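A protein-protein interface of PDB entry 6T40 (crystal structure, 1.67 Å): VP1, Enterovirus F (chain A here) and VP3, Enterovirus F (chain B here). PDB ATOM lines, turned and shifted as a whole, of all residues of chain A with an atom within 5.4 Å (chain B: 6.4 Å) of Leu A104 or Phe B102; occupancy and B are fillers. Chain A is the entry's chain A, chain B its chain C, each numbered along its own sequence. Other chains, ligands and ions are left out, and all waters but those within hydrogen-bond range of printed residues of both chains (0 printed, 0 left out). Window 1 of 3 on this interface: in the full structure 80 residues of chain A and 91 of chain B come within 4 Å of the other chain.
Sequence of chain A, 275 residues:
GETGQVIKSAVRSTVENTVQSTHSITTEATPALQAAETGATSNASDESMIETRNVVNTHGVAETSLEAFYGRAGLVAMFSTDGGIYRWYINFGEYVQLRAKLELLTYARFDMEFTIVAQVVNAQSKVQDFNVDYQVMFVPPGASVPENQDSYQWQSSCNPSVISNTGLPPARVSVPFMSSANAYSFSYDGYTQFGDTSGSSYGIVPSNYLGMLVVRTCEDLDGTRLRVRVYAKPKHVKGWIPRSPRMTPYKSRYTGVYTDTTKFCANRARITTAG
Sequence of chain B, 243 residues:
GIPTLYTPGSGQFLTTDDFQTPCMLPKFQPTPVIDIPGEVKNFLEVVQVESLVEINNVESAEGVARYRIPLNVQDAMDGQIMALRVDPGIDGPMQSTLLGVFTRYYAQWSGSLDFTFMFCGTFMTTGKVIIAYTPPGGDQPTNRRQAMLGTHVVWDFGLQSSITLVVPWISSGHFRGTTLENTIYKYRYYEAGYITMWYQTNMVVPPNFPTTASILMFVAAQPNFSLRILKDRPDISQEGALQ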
ATOM      1  N   PHE A  69      22.199 -18.958 -11.249  1.00  0.00           N
ATOM      2  CA  PHE A  69      21.468 -18.775 -12.498  1.00  0.00           C
ATOM      3  C   PHE A  69      21.950 -19.738 -13.585  1.00  0.00           C
ATOM      4  O   PHE A  69      21.146 -20.376 -14.265  1.00  0.00           O
ATOM      5  CB  PHE A  69      21.642 -17.331 -12.983  1.00  0.00           C
ATOM      6  CG  PHE A  69      20.816 -16.987 -14.193  1.00  0.00           C
ATOM      7  CD1 PHE A  69      19.490 -16.589 -14.058  1.00  0.00           C
ATOM      8  CD2 PHE A  69      21.369 -17.052 -15.470  1.00  0.00           C
ATOM      9  CE1 PHE A  69      18.722 -16.258 -15.177  1.00  0.00           C
ATOM     10  CE2 PHE A  69      20.615 -16.725 -16.597  1.00  0.00           C
ATOM     11  CZ  PHE A  69      19.286 -16.325 -16.449  1.00  0.00           C
ATOM     12  N   TYR A  70      23.267 -19.845 -13.733  1.00  0.00           N
ATOM     13  CA  TYR A  70      23.869 -20.692 -14.761  1.00  0.00           C
ATOM     14  C   TYR A  70      24.201 -22.116 -14.343  1.00  0.00           C
ATOM     15  O   TYR A  70      24.291 -23.008 -15.187  1.00  0.00           O
ATOM     16  CB  TYR A  70      25.157 -20.038 -15.269  1.00  0.00           C
ATOM     17  CG  TYR A  70      24.933 -18.791 -16.084  1.00  0.00           C
ATOM     18  CD1 TYR A  70      24.408 -18.866 -17.373  1.00  0.00           C
ATOM     19  CD2 TYR A  70      25.240 -17.532 -15.566  1.00  0.00           C
ATOM     20  CE1 TYR A  70      24.195 -17.719 -18.132  1.00  0.00           C
ATOM     21  CE2 TYR A  70      25.029 -16.374 -16.318  1.00  0.00           C
ATOM     22  CZ  TYR A  70      24.506 -16.481 -17.599  1.00  0.00           C
ATOM     23  OH  TYR A  70      24.289 -15.349 -18.348  1.00  0.00           O
ATOM     24  N   ALA A 100      20.163 -18.309 -25.044  1.00  0.00           N
ATOM     25  CA  ALA A 100      19.633 -17.030 -24.581  1.00  0.00           C
ATOM     26  C   ALA A 100      20.190 -16.649 -23.209  1.00  0.00           C
ATOM     27  O   ALA A 100      20.408 -15.468 -22.933  1.00  0.00           O
ATOM     28  CB  ALA A 100      18.106 -17.079 -24.539  1.00  0.00           C
ATOM     29  N   LYS A 101      20.418 -17.642 -22.352  1.00  0.00           N
ATOM     30  CA  LYS A 101      20.964 -17.381 -21.020  1.00  0.00           C
ATOM     31  C   LYS A 101      22.380 -16.823 -21.116  1.00  0.00           C
ATOM     32  O   LYS A 101      22.711 -15.822 -20.481  1.00  0.00           O
ATOM     33  CB  LYS A 101      21.007 -18.666 -20.182  1.00  0.00           C
ATOM     34  CG  LYS A 101      19.651 -19.247 -19.831  1.00  0.00           C
ATOM     35  CD  LYS A 101      19.790 -20.506 -18.973  1.00  0.00           C
ATOM     36  CE  LYS A 101      20.270 -20.191 -17.560  1.00  0.00           C
ATOM     37  NZ  LYS A 101      20.332 -21.427 -16.721  1.00  0.00           N
ATOM     38  N   LEU A 102      23.219 -17.481 -21.907  1.00  0.00           N
ATOM     39  CA  LEU A 102      24.602 -17.049 -22.059  1.00  0.00           C
ATOM     40  C   LEU A 102      24.722 -15.646 -22.641  1.00  0.00           C
ATOM     41  O   LEU A 102      25.606 -14.884 -22.254  1.00  0.00           O
ATOM     42  CB  LEU A 102      25.367 -18.044 -22.937  1.00  0.00           C
ATOM     43  CG  LEU A 102      25.519 -19.446 -22.338  1.00  0.00           C
ATOM     44  CD1 LEU A 102      26.141 -20.382 -23.367  1.00  0.00           C
ATOM     45  CD2 LEU A 102      26.378 -19.374 -21.082  1.00  0.00           C
ATOM     46  N   GLU A 103      23.827 -15.297 -23.560  1.00  0.00           N
ATOM     47  CA  GLU A 103      23.879 -13.982 -24.184  1.00  0.00           C
ATOM     48  C   GLU A 103      23.479 -12.824 -23.268  1.00  0.00           C
ATOM     49  O   GLU A 103      23.451 -11.669 -23.693  1.00  0.00           O
ATOM     50  CB  GLU A 103      23.056 -13.991 -25.478  1.00  0.00           C
ATOM     51  CG  GLU A 103      23.782 -14.751 -26.594  1.00  0.00           C
ATOM     52  CD  GLU A 103      22.972 -14.899 -27.871  1.00  0.00           C
ATOM     53  OE1 GLU A 103      21.983 -14.159 -28.050  1.00  0.00           O
ATOM     54  OE2 GLU A 103      23.343 -15.756 -28.706  1.00  0.00           O
ATOM     55  N   LEU A 104      23.188 -13.134 -22.007  1.00  0.00           N
ATOM     56  CA  LEU A 104      22.845 -12.104 -21.028  1.00  0.00           C
ATOM     57  C   LEU A 104      24.135 -11.457 -20.510  1.00  0.00           C
ATOM     58  O   LEU A 104      24.097 -10.454 -19.797  1.00  0.00           O
ATOM     59  CB  LEU A 104      22.068 -12.710 -19.857  1.00  0.00           C
ATOM     60  CG  LEU A 104      20.644 -13.171 -20.174  1.00  0.00           C
ATOM     61  CD1 LEU A 104      20.070 -13.940 -18.988  1.00  0.00           C
ATOM     62  CD2 LEU A 104      19.784 -11.954 -20.503  1.00  0.00           C
ATOM     63  N   LEU A 105      25.273 -12.049 -20.867  1.00  0.00           N
ATOM     64  CA  LEU A 105      26.583 -11.534 -20.467  1.00  0.00           C
ATOM     65  C   LEU A 105      27.421 -11.315 -21.721  1.00  0.00           C
ATOM     66  O   LEU A 105      27.256 -12.024 -22.710  1.00  0.00           O
ATOM     67  CB  LEU A 105      27.311 -12.537 -19.565  1.00  0.00           C
ATOM     68  CG  LEU A 105      26.747 -12.808 -18.168  1.00  0.00           C
ATOM     69  CD1 LEU A 105      27.518 -13.950 -17.519  1.00  0.00           C
ATOM     70  CD2 LEU A 105      26.847 -11.547 -17.325  1.00  0.00           C
ATOM     71  N   THR A 106      28.319 -10.337 -21.688  1.00  0.00           N
ATOM     72  CA  THR A 106      29.169 -10.087 -22.845  1.00  0.00           C
ATOM     73  C   THR A 106      30.371 -11.022 -22.782  1.00  0.00           C
ATOM     74  O   THR A 106      30.718 -11.671 -23.770  1.00  0.00           O
ATOM     75  CB  THR A 106      29.670  -8.632 -22.879  1.00  0.00           C
ATOM     76  OG1 THR A 106      28.548  -7.743 -22.850  1.00  0.00           O
ATOM     77  CG2 THR A 106      30.475  -8.376 -24.151  1.00  0.00           C
ATOM     78  N   ILE A 241      29.934  -7.277 -17.942  1.00  0.00           N
ATOM     79  CA  ILE A 241      29.092  -6.508 -18.848  1.00  0.00           C
ATOM     80  C   ILE A 241      27.761  -7.135 -19.241  1.00  0.00           C
ATOM     81  O   ILE A 241      27.639  -7.788 -20.282  1.00  0.00           O
ATOM     82  CB  ILE A 241      29.910  -6.141 -20.114  1.00  0.00           C
ATOM     83  CG1 ILE A 241      31.223  -5.476 -19.676  1.00  0.00           C
ATOM     84  CG2 ILE A 241      29.120  -5.188 -21.014  1.00  0.00           C
ATOM     85  CD1 ILE A 241      32.149  -5.096 -20.810  1.00  0.00           C
ATOM     86  N   PRO A 242      26.733  -6.933 -18.403  1.00  0.00           N
ATOM     87  CA  PRO A 242      25.389  -7.464 -18.644  1.00  0.00           C
ATOM     88  C   PRO A 242      24.878  -6.925 -19.976  1.00  0.00           C
ATOM     89  O   PRO A 242      25.172  -5.786 -20.345  1.00  0.00           O
ATOM     90  CB  PRO A 242      24.582  -6.913 -17.470  1.00  0.00           C
ATOM     91  CG  PRO A 242      25.600  -6.753 -16.393  1.00  0.00           C
ATOM     92  CD  PRO A 242      26.780  -6.184 -17.135  1.00  0.00           C
ATOM     93  N   ARG A 243      24.107  -7.733 -20.692  1.00  0.00           N
ATOM     94  CA  ARG A 243      23.582  -7.304 -21.979  1.00  0.00           C
ATOM     95  C   ARG A 243      22.065  -7.231 -22.018  1.00  0.00           C
ATOM     96  O   ARG A 243      21.369  -7.792 -21.168  1.00  0.00           O
ATOM     97  CB  ARG A 243      24.056  -8.248 -23.089  1.00  0.00           C
ATOM     98  CG  ARG A 243      25.568  -8.351 -23.232  1.00  0.00           C
ATOM     99  CD  ARG A 243      25.940  -8.984 -24.567  1.00  0.00           C
ATOM    100  NE  ARG A 243      25.649  -8.098 -25.692  1.00  0.00           N
ATOM    101  CZ  ARG A 243      26.362  -7.017 -26.001  1.00  0.00           C
ATOM    102  NH1 ARG A 243      27.420  -6.683 -25.270  1.00  0.00           N
ATOM    103  NH2 ARG A 243      26.018  -6.267 -27.041  1.00  0.00           N
ATOM    104  N   SER A 244      21.567  -6.521 -23.022  1.00  0.00           N
ATOM    105  CA  SER A 244      20.139  -6.378 -23.252  1.00  0.00           C
ATOM    106  C   SER A 244      19.689  -7.780 -23.693  1.00  0.00           C
ATOM    107  O   SER A 244      20.252  -8.346 -24.628  1.00  0.00           O
ATOM    108  CB  SER A 244      19.920  -5.351 -24.367  1.00  0.00           C
ATOM    109  OG  SER A 244      18.549  -5.103 -24.593  1.00  0.00           O
ATOM    110  N   PRO A 245      18.683  -8.363 -23.020  1.00  0.00           N
ATOM    111  CA  PRO A 245      18.186  -9.705 -23.362  1.00  0.00           C
ATOM    112  C   PRO A 245      17.618  -9.875 -24.771  1.00  0.00           C
ATOM    113  O   PRO A 245      17.075  -8.934 -25.353  1.00  0.00           O
ATOM    114  CB  PRO A 245      17.117  -9.962 -22.298  1.00  0.00           C
ATOM    115  CG  PRO A 245      17.584  -9.133 -21.130  1.00  0.00           C
ATOM    116  CD  PRO A 245      18.020  -7.856 -21.805  1.00  0.00           C
ATOM    117  N   ARG A 246      17.740 -11.086 -25.311  1.00  0.00           N
ATOM    118  CA  ARG A 246      17.203 -11.394 -26.634  1.00  0.00           C
ATOM    119  C   ARG A 246      15.704 -11.101 -26.568  1.00  0.00           C
ATOM    120  O   ARG A 246      15.039 -11.475 -25.601  1.00  0.00           O
ATOM    121  CB  ARG A 246      17.428 -12.875 -26.957  1.00  0.00           C
ATOM    122  CG  ARG A 246      16.950 -13.304 -28.340  1.00  0.00           C
ATOM    123  CD  ARG A 246      17.836 -12.743 -29.452  1.00  0.00           C
ATOM    124  NE  ARG A 246      17.381 -13.197 -30.765  1.00  0.00           N
ATOM    125  CZ  ARG A 246      18.062 -13.047 -31.897  1.00  0.00           C
ATOM    126  NH1 ARG A 246      19.247 -12.450 -31.892  1.00  0.00           N
ATOM    127  NH2 ARG A 246      17.556 -13.502 -33.036  1.00  0.00           N
ATOM    128  N   PHE B  43      22.512 -11.125 -10.690  1.00  0.00           N
ATOM    129  CA  PHE B  43      21.615 -10.410 -11.584  1.00  0.00           C
ATOM    130  C   PHE B  43      20.713  -9.385 -10.909  1.00  0.00           C
ATOM    131  O   PHE B  43      20.001  -8.646 -11.586  1.00  0.00           O
ATOM    132  CB  PHE B  43      20.810 -11.398 -12.429  1.00  0.00           C
ATOM    133  CG  PHE B  43      21.607 -11.991 -13.559  1.00  0.00           C
ATOM    134  CD1 PHE B  43      22.124 -11.170 -14.560  1.00  0.00           C
ATOM    135  CD2 PHE B  43      21.867 -13.356 -13.611  1.00  0.00           C
ATOM    136  CE1 PHE B  43      22.888 -11.700 -15.600  1.00  0.00           C
ATOM    137  CE2 PHE B  43      22.631 -13.898 -14.646  1.00  0.00           C
ATOM    138  CZ  PHE B  43      23.144 -13.068 -15.644  1.00  0.00           C
ATOM    139  N   VAL B  46      21.471  -6.139 -12.164  1.00  0.00           N
ATOM    140  CA  VAL B  46      20.903  -5.767 -13.454  1.00  0.00           C
ATOM    141  C   VAL B  46      19.456  -5.281 -13.362  1.00  0.00           C
ATOM    142  O   VAL B  46      19.103  -4.276 -13.979  1.00  0.00           O
ATOM    143  CB  VAL B  46      20.975  -6.951 -14.453  1.00  0.00           C
ATOM    144  CG1 VAL B  46      20.309  -6.573 -15.773  1.00  0.00           C
ATOM    145  CG2 VAL B  46      22.430  -7.340 -14.687  1.00  0.00           C
ATOM    146  N   VAL B  47      18.619  -5.978 -12.596  1.00  0.00           N
ATOM    147  CA  VAL B  47      17.223  -5.565 -12.487  1.00  0.00           C
ATOM    148  C   VAL B  47      17.054  -4.237 -11.755  1.00  0.00           C
ATOM    149  O   VAL B  47      15.986  -3.627 -11.814  1.00  0.00           O
ATOM    150  CB  VAL B  47      16.344  -6.643 -11.799  1.00  0.00           C
ATOM    151  CG1 VAL B  47      16.299  -7.899 -12.662  1.00  0.00           C
ATOM    152  CG2 VAL B  47      16.876  -6.959 -10.411  1.00  0.00           C
ATOM    153  N   THR B  97      11.030  -5.463 -20.448  1.00  0.00           N
ATOM    154  CA  THR B  97      11.981  -4.651 -19.685  1.00  0.00           C
ATOM    155  C   THR B  97      13.040  -5.562 -19.056  1.00  0.00           C
ATOM    156  O   THR B  97      12.871  -6.780 -19.021  1.00  0.00           O
ATOM    157  CB  THR B  97      11.284  -3.871 -18.544  1.00  0.00           C
ATOM    158  OG1 THR B  97      10.726  -4.795 -17.600  1.00  0.00           O
ATOM    159  CG2 THR B  97      10.166  -2.987 -19.097  1.00  0.00           C
ATOM    160  N   LEU B  98      14.132  -4.975 -18.571  1.00  0.00           N
ATOM    161  CA  LEU B  98      15.185  -5.760 -17.926  1.00  0.00           C
ATOM    162  C   LEU B  98      14.581  -6.464 -16.720  1.00  0.00           C
ATOM    163  O   LEU B  98      14.774  -7.663 -16.517  1.00  0.00           O
ATOM    164  CB  LEU B  98      16.324  -4.858 -17.448  1.00  0.00           C
ATOM    165  CG  LEU B  98      17.224  -4.215 -18.501  1.00  0.00           C
ATOM    166  CD1 LEU B  98      18.170  -3.231 -17.820  1.00  0.00           C
ATOM    167  CD2 LEU B  98      18.007  -5.296 -19.238  1.00  0.00           C
ATOM    168  N   LEU B  99      13.855  -5.697 -15.915  1.00  0.00           N
ATOM    169  CA  LEU B  99      13.200  -6.230 -14.730  1.00  0.00           C
ATOM    170  C   LEU B  99      12.259  -7.366 -15.122  1.00  0.00           C
ATOM    171  O   LEU B  99      12.260  -8.431 -14.504  1.00  0.00           O
ATOM    172  CB  LEU B  99      12.407  -5.122 -14.035  1.00  0.00           C
ATOM    173  CG  LEU B  99      11.499  -5.544 -12.876  1.00  0.00           C
ATOM    174  CD1 LEU B  99      12.339  -6.116 -11.742  1.00  0.00           C
ATOM    175  CD2 LEU B  99      10.700  -4.342 -12.396  1.00  0.00           C
ATOM    176  N   GLY B 100      11.462  -7.131 -16.159  1.00  0.00           N
ATOM    177  CA  GLY B 100      10.514  -8.135 -16.615  1.00  0.00           C
ATOM    178  C   GLY B 100      11.147  -9.421 -17.112  1.00  0.00           C
ATOM    179  O   GLY B 100      10.680 -10.513 -16.788  1.00  0.00           O
ATOM    180  N   VAL B 101      12.204  -9.305 -17.908  1.00  0.00           N
ATOM    181  CA  VAL B 101      12.872 -10.489 -18.433  1.00  0.00           C
ATOM    182  C   VAL B 101      13.398 -11.378 -17.312  1.00  0.00           C
ATOM    183  O   VAL B 101      13.151 -12.583 -17.298  1.00  0.00           O
ATOM    184  CB  VAL B 101      14.043 -10.108 -19.364  1.00  0.00           C
ATOM    185  CG1 VAL B 101      14.880 -11.342 -19.686  1.00  0.00           C
ATOM    186  CG2 VAL B 101      13.494  -9.500 -20.650  1.00  0.00           C
ATOM    187  N   PHE B 102      14.121 -10.793 -16.366  1.00  0.00           N
ATOM    188  CA  PHE B 102      14.655 -11.589 -15.272  1.00  0.00           C
ATOM    189  C   PHE B 102      13.562 -12.102 -14.354  1.00  0.00           C
ATOM    190  O   PHE B 102      13.651 -13.216 -13.843  1.00  0.00           O
ATOM    191  CB  PHE B 102      15.710 -10.792 -14.508  1.00  0.00           C
ATOM    192  CG  PHE B 102      17.039 -10.767 -15.206  1.00  0.00           C
ATOM    193  CD1 PHE B 102      17.880 -11.877 -15.154  1.00  0.00           C
ATOM    194  CD2 PHE B 102      17.413  -9.678 -15.986  1.00  0.00           C
ATOM    195  CE1 PHE B 102      19.072 -11.905 -15.875  1.00  0.00           C
ATOM    196  CE2 PHE B 102      18.603  -9.695 -16.712  1.00  0.00           C
ATOM    197  CZ  PHE B 102      19.435 -10.811 -16.657  1.00  0.00           C
ATOM    198  N   THR B 103      12.519 -11.307 -14.154  1.00  0.00           N
ATOM    199  CA  THR B 103      11.425 -11.764 -13.313  1.00  0.00           C
ATOM    200  C   THR B 103      10.787 -12.977 -13.994  1.00  0.00           C
ATOM    201  O   THR B 103      10.345 -13.911 -13.323  1.00  0.00           O
ATOM    202  CB  THR B 103      10.367 -10.662 -13.110  1.00  0.00           C
ATOM    203  OG1 THR B 103      10.959  -9.562 -12.406  1.00  0.00           O
ATOM    204  CG2 THR B 103       9.193 -11.193 -12.295  1.00  0.00           C
ATOM    205  N   ARG B 104      10.763 -12.973 -15.326  1.00  0.00           N
ATOM    206  CA  ARG B 104      10.179 -14.086 -16.069  1.00  0.00           C
ATOM    207  C   ARG B 104      11.067 -15.334 -16.074  1.00  0.00           C
ATOM    208  O   ARG B 104      10.662 -16.393 -16.560  1.00  0.00           O
ATOM    209  CB  ARG B 104       9.819 -13.637 -17.493  1.00  0.00           C
ATOM    210  CG  ARG B 104       8.591 -12.710 -17.502  1.00  0.00           C
ATOM    211  CD  ARG B 104       8.484 -11.877 -18.773  1.00  0.00           C
ATOM    212  NE  ARG B 104       7.926 -12.602 -19.913  1.00  0.00           N
ATOM    213  CZ  ARG B 104       6.631 -12.854 -20.087  1.00  0.00           C
ATOM    214  NH1 ARG B 104       5.739 -12.448 -19.191  1.00  0.00           N
ATOM    215  NH2 ARG B 104       6.222 -13.490 -21.178  1.00  0.00           N
ATOM    216  N   TYR B 105      12.275 -15.208 -15.529  1.00  0.00           N
ATOM    217  CA  TYR B 105      13.187 -16.346 -15.406  1.00  0.00           C
ATOM    218  C   TYR B 105      12.987 -16.960 -14.015  1.00  0.00           C
ATOM    219  O   TYR B 105      13.674 -17.912 -13.645  1.00  0.00           O
ATOM    220  CB  TYR B 105      14.651 -15.904 -15.542  1.00  0.00           C
ATOM    221  CG  TYR B 105      15.251 -16.075 -16.923  1.00  0.00           C
ATOM    222  CD1 TYR B 105      15.455 -17.345 -17.469  1.00  0.00           C
ATOM    223  CD2 TYR B 105      15.653 -14.967 -17.665  1.00  0.00           C
ATOM    224  CE1 TYR B 105      16.049 -17.504 -18.728  1.00  0.00           C
ATOM    225  CE2 TYR B 105      16.246 -15.113 -18.920  1.00  0.00           C
ATOM    226  CZ  TYR B 105      16.442 -16.381 -19.443  1.00  0.00           C
ATOM    227  OH  TYR B 105      17.037 -16.519 -20.678  1.00  0.00           O
ATOM    228  N   TYR B 106      12.053 -16.409 -13.242  1.00  0.00           N
ATOM    229  CA  TYR B 106      11.787 -16.914 -11.894  1.00  0.00           C
ATOM    230  C   TYR B 106      10.298 -17.077 -11.597  1.00  0.00           C
ATOM    231  O   TYR B 106       9.454 -16.491 -12.273  1.00  0.00           O
ATOM    232  CB  TYR B 106      12.430 -16.000 -10.843  1.00  0.00           C
ATOM    233  CG  TYR B 106      13.943 -16.053 -10.842  1.00  0.00           C
ATOM    234  CD1 TYR B 106      14.691 -15.296 -11.746  1.00  0.00           C
ATOM    235  CD2 TYR B 106      14.628 -16.895  -9.965  1.00  0.00           C
ATOM    236  CE1 TYR B 106      16.087 -15.377 -11.774  1.00  0.00           C
ATOM    237  CE2 TYR B 106      16.021 -16.985  -9.986  1.00  0.00           C
ATOM    238  CZ  TYR B 106      16.741 -16.224 -10.893  1.00  0.00           C
ATOM    239  OH  TYR B 106      18.113 -16.320 -10.924  1.00  0.00           O
ATOM    240  N   LEU B 227      14.384 -12.509  -6.163  1.00  0.00           N
ATOM    241  CA  LEU B 227      13.643 -13.486  -6.958  1.00  0.00           C
ATOM    242  C   LEU B 227      13.978 -14.900  -6.500  1.00  0.00           C
ATOM    243  O   LEU B 227      15.092 -15.157  -6.052  1.00  0.00           O
ATOM    244  CB  LEU B 227      14.017 -13.335  -8.437  1.00  0.00           C
ATOM    245  CG  LEU B 227      13.653 -12.005  -9.105  1.00  0.00           C
ATOM    246  CD1 LEU B 227      14.416 -11.852 -10.416  1.00  0.00           C
ATOM    247  CD2 LEU B 227      12.150 -11.956  -9.342  1.00  0.00           C
ATOM    248  N   ARG B 233      12.417 -18.992 -19.331  1.00  0.00           N
ATOM    249  CA  ARG B 233      11.744 -17.793 -19.809  1.00  0.00           C
ATOM    250  C   ARG B 233      10.786 -18.215 -20.926  1.00  0.00           C
ATOM    251  O   ARG B 233      11.206 -18.764 -21.942  1.00  0.00           O
ATOM    252  CB  ARG B 233      12.791 -16.806 -20.328  1.00  0.00           C
ATOM    253  CG  ARG B 233      12.234 -15.477 -20.750  1.00  0.00           C
ATOM    254  CD  ARG B 233      13.327 -14.590 -21.311  1.00  0.00           C
ATOM    255  NE  ARG B 233      12.740 -13.509 -22.090  1.00  0.00           N
ATOM    256  CZ  ARG B 233      13.403 -12.784 -22.982  1.00  0.00           C
ATOM    257  NH1 ARG B 233      14.690 -13.018 -23.208  1.00  0.00           N
ATOM    258  NH2 ARG B 233      12.766 -11.845 -23.666  1.00  0.00           N
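The guanidinium group (NH1) of Arg B233 is in hydrogen-bond range of the backbone carbonyl oxygen (O) of Arg A246 (2.9 Å).
Among the printed residues, merely in contact across the chains: Phe A69 with Phe B43, Phe A69 with Tyr B105, Phe A69 with Tyr B106, Tyr A70 with Phe B43, Lys A101 with Tyr B105, Leu A104 with Phe B102, Pro A242 with Val B46, Pro A245 with Leu B98 and Pro A245 with Val B101.
The side-chain amino group (NZ) of Lys A101 lies within hydrogen-bond range of the backbone carbonyl oxygen (O) of Phe A69 (2.8 Å).
The backbone carbonyl oxygen (O) of Lys A101 sits at hydrogen-bond distance from the side-chain hydroxyl (OH) of Tyr A70 (2.7 Å).
O of Leu A104 is in hydrogen-bond range of N of Arg A243 (2.9 Å).
Of the printed residues of chain B, Leu A104 touches Phe B102.
Phe B102 touches just one residue of chain A: Leu A104 (3.9 Å).
Of the printed residues of chain A, Val B46 touches Pro A242.
Of the printed residues of chain A, Tyr B106 touches Phe A69 (3.4 Å).
Printed residues of chain B within 4 Å of Lys A101: Tyr B105 (3.9 Å).
Of the printed residues of chain B, Phe A69 touches Phe B43 (3.5 Å), Tyr B105 (3.9 Å) and Tyr B106 (3.4 Å).
The nearest residue of chain A that does not touch Phe B102 is Phe A69 (4.4 Å).
Of the 15 printed residues of chain B, 8 touch a printed residue of chain A.
Printed residues of chain B that touch a printed residue of chain A: Phe B43, Val B46, Leu B98, Val B101, Phe B102, Tyr B105, Tyr B106 and Arg B233.
Hydrophobic or aromatic side chains of chain B that line the printed part of chain A: Phe B43, Val B46, Leu B98, Val B101, Phe B102, Tyr B105 and Tyr B106.
Hydrophobic or aromatic side chains of chain A that line the printed part of chain B: Phe A69, Tyr A70, Leu A104, Pro A242 and Pro A245.
Among the printed residues, 10 pairs touch across the chains.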
